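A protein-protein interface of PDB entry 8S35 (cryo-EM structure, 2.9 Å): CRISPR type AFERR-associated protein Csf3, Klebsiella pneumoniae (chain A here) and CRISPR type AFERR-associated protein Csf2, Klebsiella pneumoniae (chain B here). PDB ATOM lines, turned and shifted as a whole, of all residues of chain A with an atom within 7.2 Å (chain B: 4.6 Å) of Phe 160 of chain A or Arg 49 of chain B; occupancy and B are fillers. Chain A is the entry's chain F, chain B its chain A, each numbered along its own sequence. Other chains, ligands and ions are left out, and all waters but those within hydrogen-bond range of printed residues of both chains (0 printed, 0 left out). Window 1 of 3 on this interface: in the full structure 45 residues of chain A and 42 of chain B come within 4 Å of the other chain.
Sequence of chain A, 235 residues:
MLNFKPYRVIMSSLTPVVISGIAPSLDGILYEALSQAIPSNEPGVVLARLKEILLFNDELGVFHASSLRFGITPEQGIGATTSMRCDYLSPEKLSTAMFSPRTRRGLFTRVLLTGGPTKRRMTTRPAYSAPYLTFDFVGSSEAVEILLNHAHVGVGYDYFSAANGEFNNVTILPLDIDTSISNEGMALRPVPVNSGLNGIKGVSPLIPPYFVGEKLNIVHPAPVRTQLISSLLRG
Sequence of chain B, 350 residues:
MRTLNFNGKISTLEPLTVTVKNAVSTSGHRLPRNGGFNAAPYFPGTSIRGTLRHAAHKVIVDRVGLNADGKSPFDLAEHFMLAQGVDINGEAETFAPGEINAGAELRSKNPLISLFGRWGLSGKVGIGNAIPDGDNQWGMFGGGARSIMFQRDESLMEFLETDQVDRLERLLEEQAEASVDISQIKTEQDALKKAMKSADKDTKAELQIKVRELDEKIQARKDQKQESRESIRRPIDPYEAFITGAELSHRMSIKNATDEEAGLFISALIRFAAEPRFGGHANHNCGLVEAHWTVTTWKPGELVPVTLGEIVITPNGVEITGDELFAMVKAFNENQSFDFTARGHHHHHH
The backbone carbonyl oxygen (O) of Gly 126 of chain B lies within hydrogen-bond range of a ring nitrogen (NE2) of His 152 of chain A, at 2.9 Å.
N of Ile 127 of chain B is in hydrogen-bond range of O of Phe 160 of chain A, 3.5 Å away.
NH2 of Arg 49 of chain B is in hydrogen-bond range of O of Val 125 of chain B, at 2.6 Å.
The backbone carbonyl oxygen (O) of Leu 115 of chain B lies within hydrogen-bond range of the backbone NH (N) of Lys 124 of chain B (2.6 Å).
The backbone carbonyl oxygen of Leu 115 of chain B sits at hydrogen-bond distance from the backbone NH of Val 125 of chain B (2.6 Å).
The backbone carbonyl oxygen (O) of Lys 124 of chain B is in hydrogen-bond range of the backbone NH (N) of Lys 255 of chain B, at 2.9 Å.
The side-chain hydroxyl (OH) of Tyr 159 of chain A lies close to a ring nitrogen (ND1) of His 152 of chain A, 3.2 Å away.
O of Asp 158 of chain A is in hydrogen-bond range of N of Ala 163 of chain A, 3.3 Å away.
Among the printed residues, pairs that only touch across the chains: Phe 160 of chain A with Gly 126 of chain B, Phe 160 of chain A with Lys 124 of chain B, Arg 85 of chain A with Thr 46 of chain B, Ser 161 of chain A with Arg 49 of chain B, Ala 163 of chain A with Ile 127 of chain B, Phe 160 of chain A with Val 125 of chain B, Ala 162 of chain A with Thr 46 of chain B, Glu 32 of chain A with Lys 255 of chain B, Gln 36 of chain A with Lys 255 of chain B, Phe 160 of chain A with Lys 255 of chain B, Ala 163 of chain A with Gly 45 of chain B, His 152 of chain A with Ile 127 of chain B, Phe 160 of chain A with Gly 123 of chain B and Phe 160 of chain A with Arg 49 of chain B.
Of the printed residues of chain B, Gln 36 of chain A touches Lys 255.
Printed residues of chain B within 4 Å of His 152 of chain A: Gly 126 and Ile 127.
Of the printed residues of chain B, Phe 160 of chain A touches Arg 49 (3.999 Å), Gly 123 (3.98 Å), Lys 124 (3.1 Å), Val 125 (3.4 Å), Gly 126 (3.1 Å), Ile 127 (3.5 Å) and Lys 255 (3.7 Å).
Printed residues of chain B within 4 Å of Ser 161 of chain A: Arg 49 (3.1 Å).
Ile 48 of chain B touches none of the printed residues of chain A.
Printed residues of chain A within 4 Å of Arg 49 of chain B: Phe 160 and Ser 161.
Of the printed residues of chain A, Val 125 of chain B touches Phe 160.
Of the printed residues of chain A, Ile 127 of chain B touches His 152, Phe 160 and Ala 163.
The nearest printed residue of chain A that does not touch Arg 49 of chain B is Arg 85 of chain A (4.4 Å).
Hydrophobic or aromatic side chains of chain A that line the printed part of chain B: His 152, Phe 160 and Ala 163.
Along chain A the printed residues that touch a printed residue of chain B span positions 32 to 163.
Among the printed residues, no Asp or Glu carboxylate lies within 4 Å of a Lys or Arg side-chain nitrogen of the other chain.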
ATOM      1  N   GLU A  32     -30.985  -9.366 -20.741  1.00  0.00           N
ATOM      2  CA  GLU A  32     -30.497 -10.668 -21.183  1.00  0.00           C
ATOM      3  C   GLU A  32     -31.049 -11.013 -22.559  1.00  0.00           C
ATOM      4  O   GLU A  32     -30.331 -11.545 -23.416  1.00  0.00           O
ATOM      5  CB  GLU A  32     -30.879 -11.746 -20.170  1.00  0.00           C
ATOM      6  CG  GLU A  32     -30.293 -13.124 -20.466  1.00  0.00           C
ATOM      7  CD  GLU A  32     -28.783 -13.152 -20.361  1.00  0.00           C
ATOM      8  OE1 GLU A  32     -28.213 -12.234 -19.733  1.00  0.00           O
ATOM      9  OE2 GLU A  32     -28.165 -14.089 -20.907  1.00  0.00           O
ATOM     10  N   GLN A  36     -28.869 -11.643 -25.964  1.00  0.00           N
ATOM     11  CA  GLN A  36     -29.042 -12.738 -26.909  1.00  0.00           C
ATOM     12  C   GLN A  36     -29.319 -12.210 -28.312  1.00  0.00           C
ATOM     13  O   GLN A  36     -28.750 -12.705 -29.291  1.00  0.00           O
ATOM     14  CB  GLN A  36     -30.173 -13.653 -26.449  1.00  0.00           C
ATOM     15  CG  GLN A  36     -29.761 -14.638 -25.376  1.00  0.00           C
ATOM     16  CD  GLN A  36     -30.948 -15.224 -24.643  1.00  0.00           C
ATOM     17  OE1 GLN A  36     -31.955 -15.585 -25.253  1.00  0.00           O
ATOM     18  NE2 GLN A  36     -30.841 -15.316 -23.324  1.00  0.00           N
ATOM     19  N   ARG A  85     -30.314 -29.055  -7.939  1.00  0.00           N
ATOM     20  CA  ARG A  85     -29.265 -29.379  -8.896  1.00  0.00           C
ATOM     21  C   ARG A  85     -28.287 -30.352  -8.258  1.00  0.00           C
ATOM     22  O   ARG A  85     -27.748 -30.082  -7.177  1.00  0.00           O
ATOM     23  CB  ARG A  85     -28.538 -28.114  -9.351  1.00  0.00           C
ATOM     24  CG  ARG A  85     -29.407 -27.158 -10.146  1.00  0.00           C
ATOM     25  CD  ARG A  85     -28.720 -26.714 -11.424  1.00  0.00           C
ATOM     26  NE  ARG A  85     -28.534 -27.815 -12.360  1.00  0.00           N
ATOM     27  CZ  ARG A  85     -27.892 -27.719 -13.517  1.00  0.00           C
ATOM     28  NH1 ARG A  85     -27.360 -26.577 -13.925  1.00  0.00           N
ATOM     29  NH2 ARG A  85     -27.778 -28.799 -14.285  1.00  0.00           N
ATOM     30  N   HIS A 152     -34.230 -16.569 -25.120  1.00  0.00           N
ATOM     31  CA  HIS A 152     -34.074 -17.575 -24.071  1.00  0.00           C
ATOM     32  C   HIS A 152     -33.831 -16.869 -22.742  1.00  0.00           C
ATOM     33  O   HIS A 152     -32.711 -16.793 -22.231  1.00  0.00           O
ATOM     34  CB  HIS A 152     -32.944 -18.534 -24.411  1.00  0.00           C
ATOM     35  CG  HIS A 152     -32.959 -19.790 -23.601  1.00  0.00           C
ATOM     36  ND1 HIS A 152     -33.931 -20.756 -23.746  1.00  0.00           N
ATOM     37  CD2 HIS A 152     -32.121 -20.240 -22.639  1.00  0.00           C
ATOM     38  CE1 HIS A 152     -33.690 -21.747 -22.907  1.00  0.00           C
ATOM     39  NE2 HIS A 152     -32.600 -21.459 -22.222  1.00  0.00           N
ATOM     40  N   VAL A 153     -34.911 -16.343 -22.175  1.00  0.00           N
ATOM     41  CA  VAL A 153     -34.869 -15.604 -20.921  1.00  0.00           C
ATOM     42  C   VAL A 153     -35.978 -16.105 -20.014  1.00  0.00           C
ATOM     43  O   VAL A 153     -37.106 -16.337 -20.463  1.00  0.00           O
ATOM     44  CB  VAL A 153     -35.007 -14.085 -21.145  1.00  0.00           C
ATOM     45  CG1 VAL A 153     -33.907 -13.591 -22.054  1.00  0.00           C
ATOM     46  CG2 VAL A 153     -36.379 -13.744 -21.715  1.00  0.00           C
ATOM     47  N   GLY A 154     -35.651 -16.284 -18.734  1.00  0.00           N
ATOM     48  CA  GLY A 154     -36.625 -16.657 -17.732  1.00  0.00           C
ATOM     49  C   GLY A 154     -36.584 -15.695 -16.561  1.00  0.00           C
ATOM     50  O   GLY A 154     -35.832 -14.718 -16.557  1.00  0.00           O
ATOM     51  N   TYR A 157     -33.003 -16.824 -10.860  1.00  0.00           N
ATOM     52  CA  TYR A 157     -31.556 -16.712 -10.724  1.00  0.00           C
ATOM     53  C   TYR A 157     -30.833 -17.203 -11.974  1.00  0.00           C
ATOM     54  O   TYR A 157     -30.089 -16.445 -12.603  1.00  0.00           O
ATOM     55  CB  TYR A 157     -31.098 -17.479  -9.479  1.00  0.00           C
ATOM     56  CG  TYR A 157     -29.647 -17.904  -9.477  1.00  0.00           C
ATOM     57  CD1 TYR A 157     -28.629 -16.978  -9.634  1.00  0.00           C
ATOM     58  CD2 TYR A 157     -29.296 -19.223  -9.244  1.00  0.00           C
ATOM     59  CE1 TYR A 157     -27.308 -17.367  -9.617  1.00  0.00           C
ATOM     60  CE2 TYR A 157     -27.981 -19.621  -9.230  1.00  0.00           C
ATOM     61  CZ  TYR A 157     -26.989 -18.690  -9.411  1.00  0.00           C
ATOM     62  OH  TYR A 157     -25.671 -19.080  -9.387  1.00  0.00           O
ATOM     63  N   ASP A 158     -31.035 -18.468 -12.350  1.00  0.00           N
ATOM     64  CA  ASP A 158     -30.374 -19.045 -13.522  1.00  0.00           C
ATOM     65  C   ASP A 158     -31.437 -19.702 -14.388  1.00  0.00           C
ATOM     66  O   ASP A 158     -31.721 -20.891 -14.228  1.00  0.00           O
ATOM     67  CB  ASP A 158     -29.312 -20.056 -13.121  1.00  0.00           C
ATOM     68  CG  ASP A 158     -29.734 -20.895 -11.944  1.00  0.00           C
ATOM     69  OD1 ASP A 158     -30.759 -20.553 -11.319  1.00  0.00           O
ATOM     70  OD2 ASP A 158     -29.040 -21.885 -11.631  1.00  0.00           O
ATOM     71  N   TYR A 159     -32.027 -18.938 -15.303  1.00  0.00           N
ATOM     72  CA  TYR A 159     -32.826 -19.581 -16.331  1.00  0.00           C
ATOM     73  C   TYR A 159     -31.933 -20.244 -17.362  1.00  0.00           C
ATOM     74  O   TYR A 159     -32.298 -21.274 -17.932  1.00  0.00           O
ATOM     75  CB  TYR A 159     -33.743 -18.582 -17.025  1.00  0.00           C
ATOM     76  CG  TYR A 159     -34.400 -19.176 -18.244  1.00  0.00           C
ATOM     77  CD1 TYR A 159     -35.398 -20.127 -18.114  1.00  0.00           C
ATOM     78  CD2 TYR A 159     -34.022 -18.796 -19.521  1.00  0.00           C
ATOM     79  CE1 TYR A 159     -36.004 -20.680 -19.217  1.00  0.00           C
ATOM     80  CE2 TYR A 159     -34.627 -19.340 -20.629  1.00  0.00           C
ATOM     81  CZ  TYR A 159     -35.616 -20.281 -20.473  1.00  0.00           C
ATOM     82  OH  TYR A 159     -36.217 -20.830 -21.579  1.00  0.00           O
ATOM     83  N   PHE A 160     -30.767 -19.657 -17.621  1.00  0.00           N
ATOM     84  CA  PHE A 160     -29.867 -20.225 -18.614  1.00  0.00           C
ATOM     85  C   PHE A 160     -29.355 -21.590 -18.176  1.00  0.00           C
ATOM     86  O   PHE A 160     -29.486 -22.577 -18.908  1.00  0.00           O
ATOM     87  CB  PHE A 160     -28.710 -19.262 -18.864  1.00  0.00           C
ATOM     88  CG  PHE A 160     -28.436 -19.027 -20.308  1.00  0.00           C
ATOM     89  CD1 PHE A 160     -29.159 -18.084 -21.011  1.00  0.00           C
ATOM     90  CD2 PHE A 160     -27.457 -19.740 -20.963  1.00  0.00           C
ATOM     91  CE1 PHE A 160     -28.915 -17.865 -22.342  1.00  0.00           C
ATOM     92  CE2 PHE A 160     -27.208 -19.518 -22.292  1.00  0.00           C
ATOM     93  CZ  PHE A 160     -27.938 -18.583 -22.983  1.00  0.00           C
ATOM     94  N   SER A 161     -28.790 -21.676 -16.973  1.00  0.00           N
ATOM     95  CA  SER A 161     -28.209 -22.937 -16.524  1.00  0.00           C
ATOM     96  C   SER A 161     -29.268 -23.889 -15.980  1.00  0.00           C
ATOM     97  O   SER A 161     -29.447 -24.996 -16.496  1.00  0.00           O
ATOM     98  CB  SER A 161     -27.144 -22.668 -15.458  1.00  0.00           C
ATOM     99  OG  SER A 161     -26.885 -23.834 -14.697  1.00  0.00           O
ATOM    100  N   ALA A 162     -29.989 -23.466 -14.945  1.00  0.00           N
ATOM    101  CA  ALA A 162     -30.925 -24.348 -14.261  1.00  0.00           C
ATOM    102  C   ALA A 162     -32.285 -24.443 -14.937  1.00  0.00           C
ATOM    103  O   ALA A 162     -33.080 -25.307 -14.557  1.00  0.00           O
ATOM    104  CB  ALA A 162     -31.115 -23.887 -12.816  1.00  0.00           C
ATOM    105  N   ALA A 163     -32.579 -23.585 -15.912  1.00  0.00           N
ATOM    106  CA  ALA A 163     -33.896 -23.549 -16.542  1.00  0.00           C
ATOM    107  C   ALA A 163     -34.983 -23.221 -15.525  1.00  0.00           C
ATOM    108  O   ALA A 163     -36.114 -23.700 -15.632  1.00  0.00           O
ATOM    109  CB  ALA A 163     -34.210 -24.871 -17.247  1.00  0.00           C
ATOM    110  N   ASN A 164     -34.647 -22.407 -14.530  1.00  0.00           N
ATOM    111  CA  ASN A 164     -35.612 -22.017 -13.515  1.00  0.00           C
ATOM    112  C   ASN A 164     -36.526 -20.920 -14.038  1.00  0.00           C
ATOM    113  O   ASN A 164     -36.099 -20.031 -14.777  1.00  0.00           O
ATOM    114  CB  ASN A 164     -34.898 -21.533 -12.253  1.00  0.00           C
ATOM    115  CG  ASN A 164     -34.382 -22.672 -11.396  1.00  0.00           C
ATOM    116  OD1 ASN A 164     -33.199 -22.722 -11.065  1.00  0.00           O
ATOM    117  ND2 ASN A 164     -35.267 -23.588 -11.023  1.00  0.00           N
ATOM    118  N   GLY B  45     -34.976 -28.877 -17.110  1.00  0.00           N
ATOM    119  CA  GLY B  45     -33.933 -28.520 -18.043  1.00  0.00           C
ATOM    120  C   GLY B  45     -32.555 -28.848 -17.530  1.00  0.00           C
ATOM    121  O   GLY B  45     -31.609 -28.906 -18.318  1.00  0.00           O
ATOM    122  N   THR B  46     -32.424 -29.070 -16.221  1.00  0.00           N
ATOM    123  CA  THR B  46     -31.155 -29.524 -15.672  1.00  0.00           C
ATOM    124  C   THR B  46     -30.805 -30.911 -16.189  1.00  0.00           C
ATOM    125  O   THR B  46     -29.651 -31.175 -16.538  1.00  0.00           O
ATOM    126  CB  THR B  46     -31.213 -29.523 -14.146  1.00  0.00           C
ATOM    127  OG1 THR B  46     -32.315 -30.326 -13.706  1.00  0.00           O
ATOM    128  CG2 THR B  46     -31.385 -28.110 -13.623  1.00  0.00           C
ATOM    129  N   SER B  47     -31.787 -31.813 -16.237  1.00  0.00           N
ATOM    130  CA  SER B  47     -31.519 -33.162 -16.721  1.00  0.00           C
ATOM    131  C   SER B  47     -31.128 -33.150 -18.191  1.00  0.00           C
ATOM    132  O   SER B  47     -30.168 -33.815 -18.596  1.00  0.00           O
ATOM    133  CB  SER B  47     -32.743 -34.049 -16.499  1.00  0.00           C
ATOM    134  OG  SER B  47     -32.573 -35.306 -17.127  1.00  0.00           O
ATOM    135  N   ILE B  48     -31.861 -32.395 -19.010  1.00  0.00           N
ATOM    136  CA  ILE B  48     -31.518 -32.317 -20.425  1.00  0.00           C
ATOM    137  C   ILE B  48     -30.161 -31.649 -20.595  1.00  0.00           C
ATOM    138  O   ILE B  48     -29.366 -32.037 -21.457  1.00  0.00           O
ATOM    139  CB  ILE B  48     -32.614 -31.578 -21.216  1.00  0.00           C
ATOM    140  CG1 ILE B  48     -33.981 -32.249 -21.032  1.00  0.00           C
ATOM    141  CG2 ILE B  48     -32.259 -31.532 -22.704  1.00  0.00           C
ATOM    142  CD1 ILE B  48     -35.143 -31.410 -21.524  1.00  0.00           C
ATOM    143  N   ARG B  49     -29.871 -30.645 -19.769  1.00  0.00           N
ATOM    144  CA  ARG B  49     -28.584 -29.967 -19.849  1.00  0.00           C
ATOM    145  C   ARG B  49     -27.449 -30.923 -19.532  1.00  0.00           C
ATOM    146  O   ARG B  49     -26.433 -30.947 -20.228  1.00  0.00           O
ATOM    147  CB  ARG B  49     -28.556 -28.775 -18.895  1.00  0.00           C
ATOM    148  CG  ARG B  49     -27.296 -27.934 -19.008  1.00  0.00           C
ATOM    149  CD  ARG B  49     -27.436 -26.604 -18.289  1.00  0.00           C
ATOM    150  NE  ARG B  49     -26.782 -25.521 -19.013  1.00  0.00           N
ATOM    151  CZ  ARG B  49     -25.470 -25.336 -19.066  1.00  0.00           C
ATOM    152  NH1 ARG B  49     -24.628 -26.149 -18.448  1.00  0.00           N
ATOM    153  NH2 ARG B  49     -24.990 -24.308 -19.757  1.00  0.00           N
ATOM    154  N   GLY B  50     -27.605 -31.721 -18.478  1.00  0.00           N
ATOM    155  CA  GLY B  50     -26.565 -32.670 -18.129  1.00  0.00           C
ATOM    156  C   GLY B  50     -26.409 -33.761 -19.170  1.00  0.00           C
ATOM    157  O   GLY B  50     -25.291 -34.173 -19.484  1.00  0.00           O
ATOM    158  N   THR B  51     -27.525 -34.236 -19.727  1.00  0.00           N
ATOM    159  CA  THR B  51     -27.444 -35.248 -20.773  1.00  0.00           C
ATOM    160  C   THR B  51     -26.718 -34.705 -21.995  1.00  0.00           C
ATOM    161  O   THR B  51     -25.843 -35.374 -22.557  1.00  0.00           O
ATOM    162  CB  THR B  51     -28.843 -35.730 -21.153  1.00  0.00           C
ATOM    163  OG1 THR B  51     -29.573 -36.070 -19.969  1.00  0.00           O
ATOM    164  CG2 THR B  51     -28.760 -36.947 -22.060  1.00  0.00           C
ATOM    165  N   LEU B  52     -27.051 -33.484 -22.411  1.00  0.00           N
ATOM    166  CA  LEU B  52     -26.399 -32.913 -23.580  1.00  0.00           C
ATOM    167  C   LEU B  52     -24.949 -32.559 -23.288  1.00  0.00           C
ATOM    168  O   LEU B  52     -24.101 -32.658 -24.176  1.00  0.00           O
ATOM    169  CB  LEU B  52     -27.161 -31.680 -24.055  1.00  0.00           C
ATOM    170  CG  LEU B  52     -28.555 -31.970 -24.612  1.00  0.00           C
ATOM    171  CD1 LEU B  52     -29.405 -30.714 -24.601  1.00  0.00           C
ATOM    172  CD2 LEU B  52     -28.464 -32.546 -26.012  1.00  0.00           C
ATOM    173  N   ARG B  53     -24.642 -32.150 -22.056  1.00  0.00           N
ATOM    174  CA  ARG B  53     -23.255 -31.904 -21.691  1.00  0.00           C
ATOM    175  C   ARG B  53     -22.447 -33.191 -21.729  1.00  0.00           C
ATOM    176  O   ARG B  53     -21.302 -33.198 -22.190  1.00  0.00           O
ATOM    177  CB  ARG B  53     -23.182 -31.260 -20.309  1.00  0.00           C
ATOM    178  CG  ARG B  53     -21.782 -30.874 -19.886  1.00  0.00           C
ATOM    179  CD  ARG B  53     -21.799 -30.015 -18.637  1.00  0.00           C
ATOM    180  NE  ARG B  53     -20.453 -29.783 -18.130  1.00  0.00           N
ATOM    181  CZ  ARG B  53     -19.982 -28.597 -17.775  1.00  0.00           C
ATOM    182  NH1 ARG B  53     -20.727 -27.506 -17.850  1.00  0.00           N
ATOM    183  NH2 ARG B  53     -18.732 -28.501 -17.334  1.00  0.00           N
ATOM    184  N   LEU B 115     -19.476 -23.684 -24.480  1.00  0.00           N
ATOM    185  CA  LEU B 115     -20.904 -23.948 -24.618  1.00  0.00           C
ATOM    186  C   LEU B 115     -21.564 -24.103 -23.257  1.00  0.00           C
ATOM    187  O   LEU B 115     -22.448 -23.323 -22.885  1.00  0.00           O
ATOM    188  CB  LEU B 115     -21.107 -25.208 -25.456  1.00  0.00           C
ATOM    189  CG  LEU B 115     -20.970 -25.060 -26.971  1.00  0.00           C
ATOM    190  CD1 LEU B 115     -20.840 -26.430 -27.598  1.00  0.00           C
ATOM    191  CD2 LEU B 115     -22.141 -24.309 -27.586  1.00  0.00           C
ATOM    192  N   PHE B 116     -21.138 -25.103 -22.496  1.00  0.00           N
ATOM    193  CA  PHE B 116     -21.506 -25.240 -21.099  1.00  0.00           C
ATOM    194  C   PHE B 116     -20.396 -24.621 -20.268  1.00  0.00           C
ATOM    195  O   PHE B 116     -19.214 -24.822 -20.555  1.00  0.00           O
ATOM    196  CB  PHE B 116     -21.705 -26.706 -20.721  1.00  0.00           C
ATOM    197  CG  PHE B 116     -22.421 -27.503 -21.766  1.00  0.00           C
ATOM    198  CD1 PHE B 116     -23.802 -27.523 -21.816  1.00  0.00           C
ATOM    199  CD2 PHE B 116     -21.715 -28.230 -22.705  1.00  0.00           C
ATOM    200  CE1 PHE B 116     -24.463 -28.254 -22.777  1.00  0.00           C
ATOM    201  CE2 PHE B 116     -22.371 -28.962 -23.669  1.00  0.00           C
ATOM    202  CZ  PHE B 116     -23.747 -28.975 -23.704  1.00  0.00           C
ATOM    203  N   GLY B 117     -20.769 -23.895 -19.233  1.00  0.00           N
ATOM    204  CA  GLY B 117     -19.775 -23.187 -18.464  1.00  0.00           C
ATOM    205  C   GLY B 117     -19.070 -24.073 -17.466  1.00  0.00           C
ATOM    206  O   GLY B 117     -19.459 -25.211 -17.211  1.00  0.00           O
ATOM    207  N   GLY B 123     -21.779 -20.243 -18.877  1.00  0.00           N
ATOM    208  CA  GLY B 123     -21.987 -21.077 -20.037  1.00  0.00           C
ATOM    209  C   GLY B 123     -22.738 -20.346 -21.130  1.00  0.00           C
ATOM    210  O   GLY B 123     -23.489 -19.400 -20.889  1.00  0.00           O
ATOM    211  N   LYS B 124     -22.530 -20.804 -22.362  1.00  0.00           N
ATOM    212  CA  LYS B 124     -23.173 -20.201 -23.520  1.00  0.00           C
ATOM    213  C   LYS B 124     -24.457 -20.910 -23.917  1.00  0.00           C
ATOM    214  O   LYS B 124     -25.284 -20.311 -24.612  1.00  0.00           O
ATOM    215  CB  LYS B 124     -22.221 -20.192 -24.717  1.00  0.00           C
ATOM    216  CG  LYS B 124     -21.396 -18.926 -24.832  1.00  0.00           C
ATOM    217  CD  LYS B 124     -20.542 -18.936 -26.084  1.00  0.00           C
ATOM    218  CE  LYS B 124     -19.646 -17.715 -26.149  1.00  0.00           C
ATOM    219  NZ  LYS B 124     -18.595 -17.846 -27.194  1.00  0.00           N
ATOM    220  N   VAL B 125     -24.637 -22.160 -23.506  1.00  0.00           N
ATOM    221  CA  VAL B 125     -25.813 -22.946 -23.857  1.00  0.00           C
ATOM    222  C   VAL B 125     -26.815 -22.865 -22.716  1.00  0.00           C
ATOM    223  O   VAL B 125     -26.504 -23.215 -21.572  1.00  0.00           O
ATOM    224  CB  VAL B 125     -25.443 -24.405 -24.160  1.00  0.00           C
ATOM    225  CG1 VAL B 125     -26.674 -25.201 -24.525  1.00  0.00           C
ATOM    226  CG2 VAL B 125     -24.470 -24.460 -25.303  1.00  0.00           C
ATOM    227  N   GLY B 126     -28.018 -22.407 -23.041  1.00  0.00           N
ATOM    228  CA  GLY B 126     -29.142 -22.370 -22.135  1.00  0.00           C
ATOM    229  C   GLY B 126     -30.153 -23.432 -22.506  1.00  0.00           C
ATOM    230  O   GLY B 126     -30.816 -23.317 -23.540  1.00  0.00           O
ATOM    231  N   ILE B 127     -30.274 -24.471 -21.689  1.00  0.00           N
ATOM    232  CA  ILE B 127     -31.128 -25.613 -21.987  1.00  0.00           C
ATOM    233  C   ILE B 127     -32.392 -25.462 -21.157  1.00  0.00           C
ATOM    234  O   ILE B 127     -32.367 -25.631 -19.933  1.00  0.00           O
ATOM    235  CB  ILE B 127     -30.426 -26.940 -21.667  1.00  0.00           C
ATOM    236  CG1 ILE B 127     -29.116 -27.082 -22.451  1.00  0.00           C
ATOM    237  CG2 ILE B 127     -31.356 -28.113 -21.926  1.00  0.00           C
ATOM    238  CD1 ILE B 127     -29.274 -27.149 -23.950  1.00  0.00           C
ATOM    239  N   LYS B 255     -25.771 -18.677 -26.926  1.00  0.00           N
ATOM    240  CA  LYS B 255     -25.674 -17.224 -26.884  1.00  0.00           C
ATOM    241  C   LYS B 255     -24.340 -16.763 -27.451  1.00  0.00           C
ATOM    242  O   LYS B 255     -23.285 -17.225 -27.006  1.00  0.00           O
ATOM    243  CB  LYS B 255     -25.826 -16.728 -25.445  1.00  0.00           C
ATOM    244  CG  LYS B 255     -26.094 -15.245 -25.302  1.00  0.00           C
ATOM    245  CD  LYS B 255     -26.344 -14.886 -23.846  1.00  0.00           C
ATOM    246  CE  LYS B 255     -26.040 -13.426 -23.566  1.00  0.00           C
ATOM    247  NZ  LYS B 255     -24.577 -13.150 -23.579  1.00  0.00           N
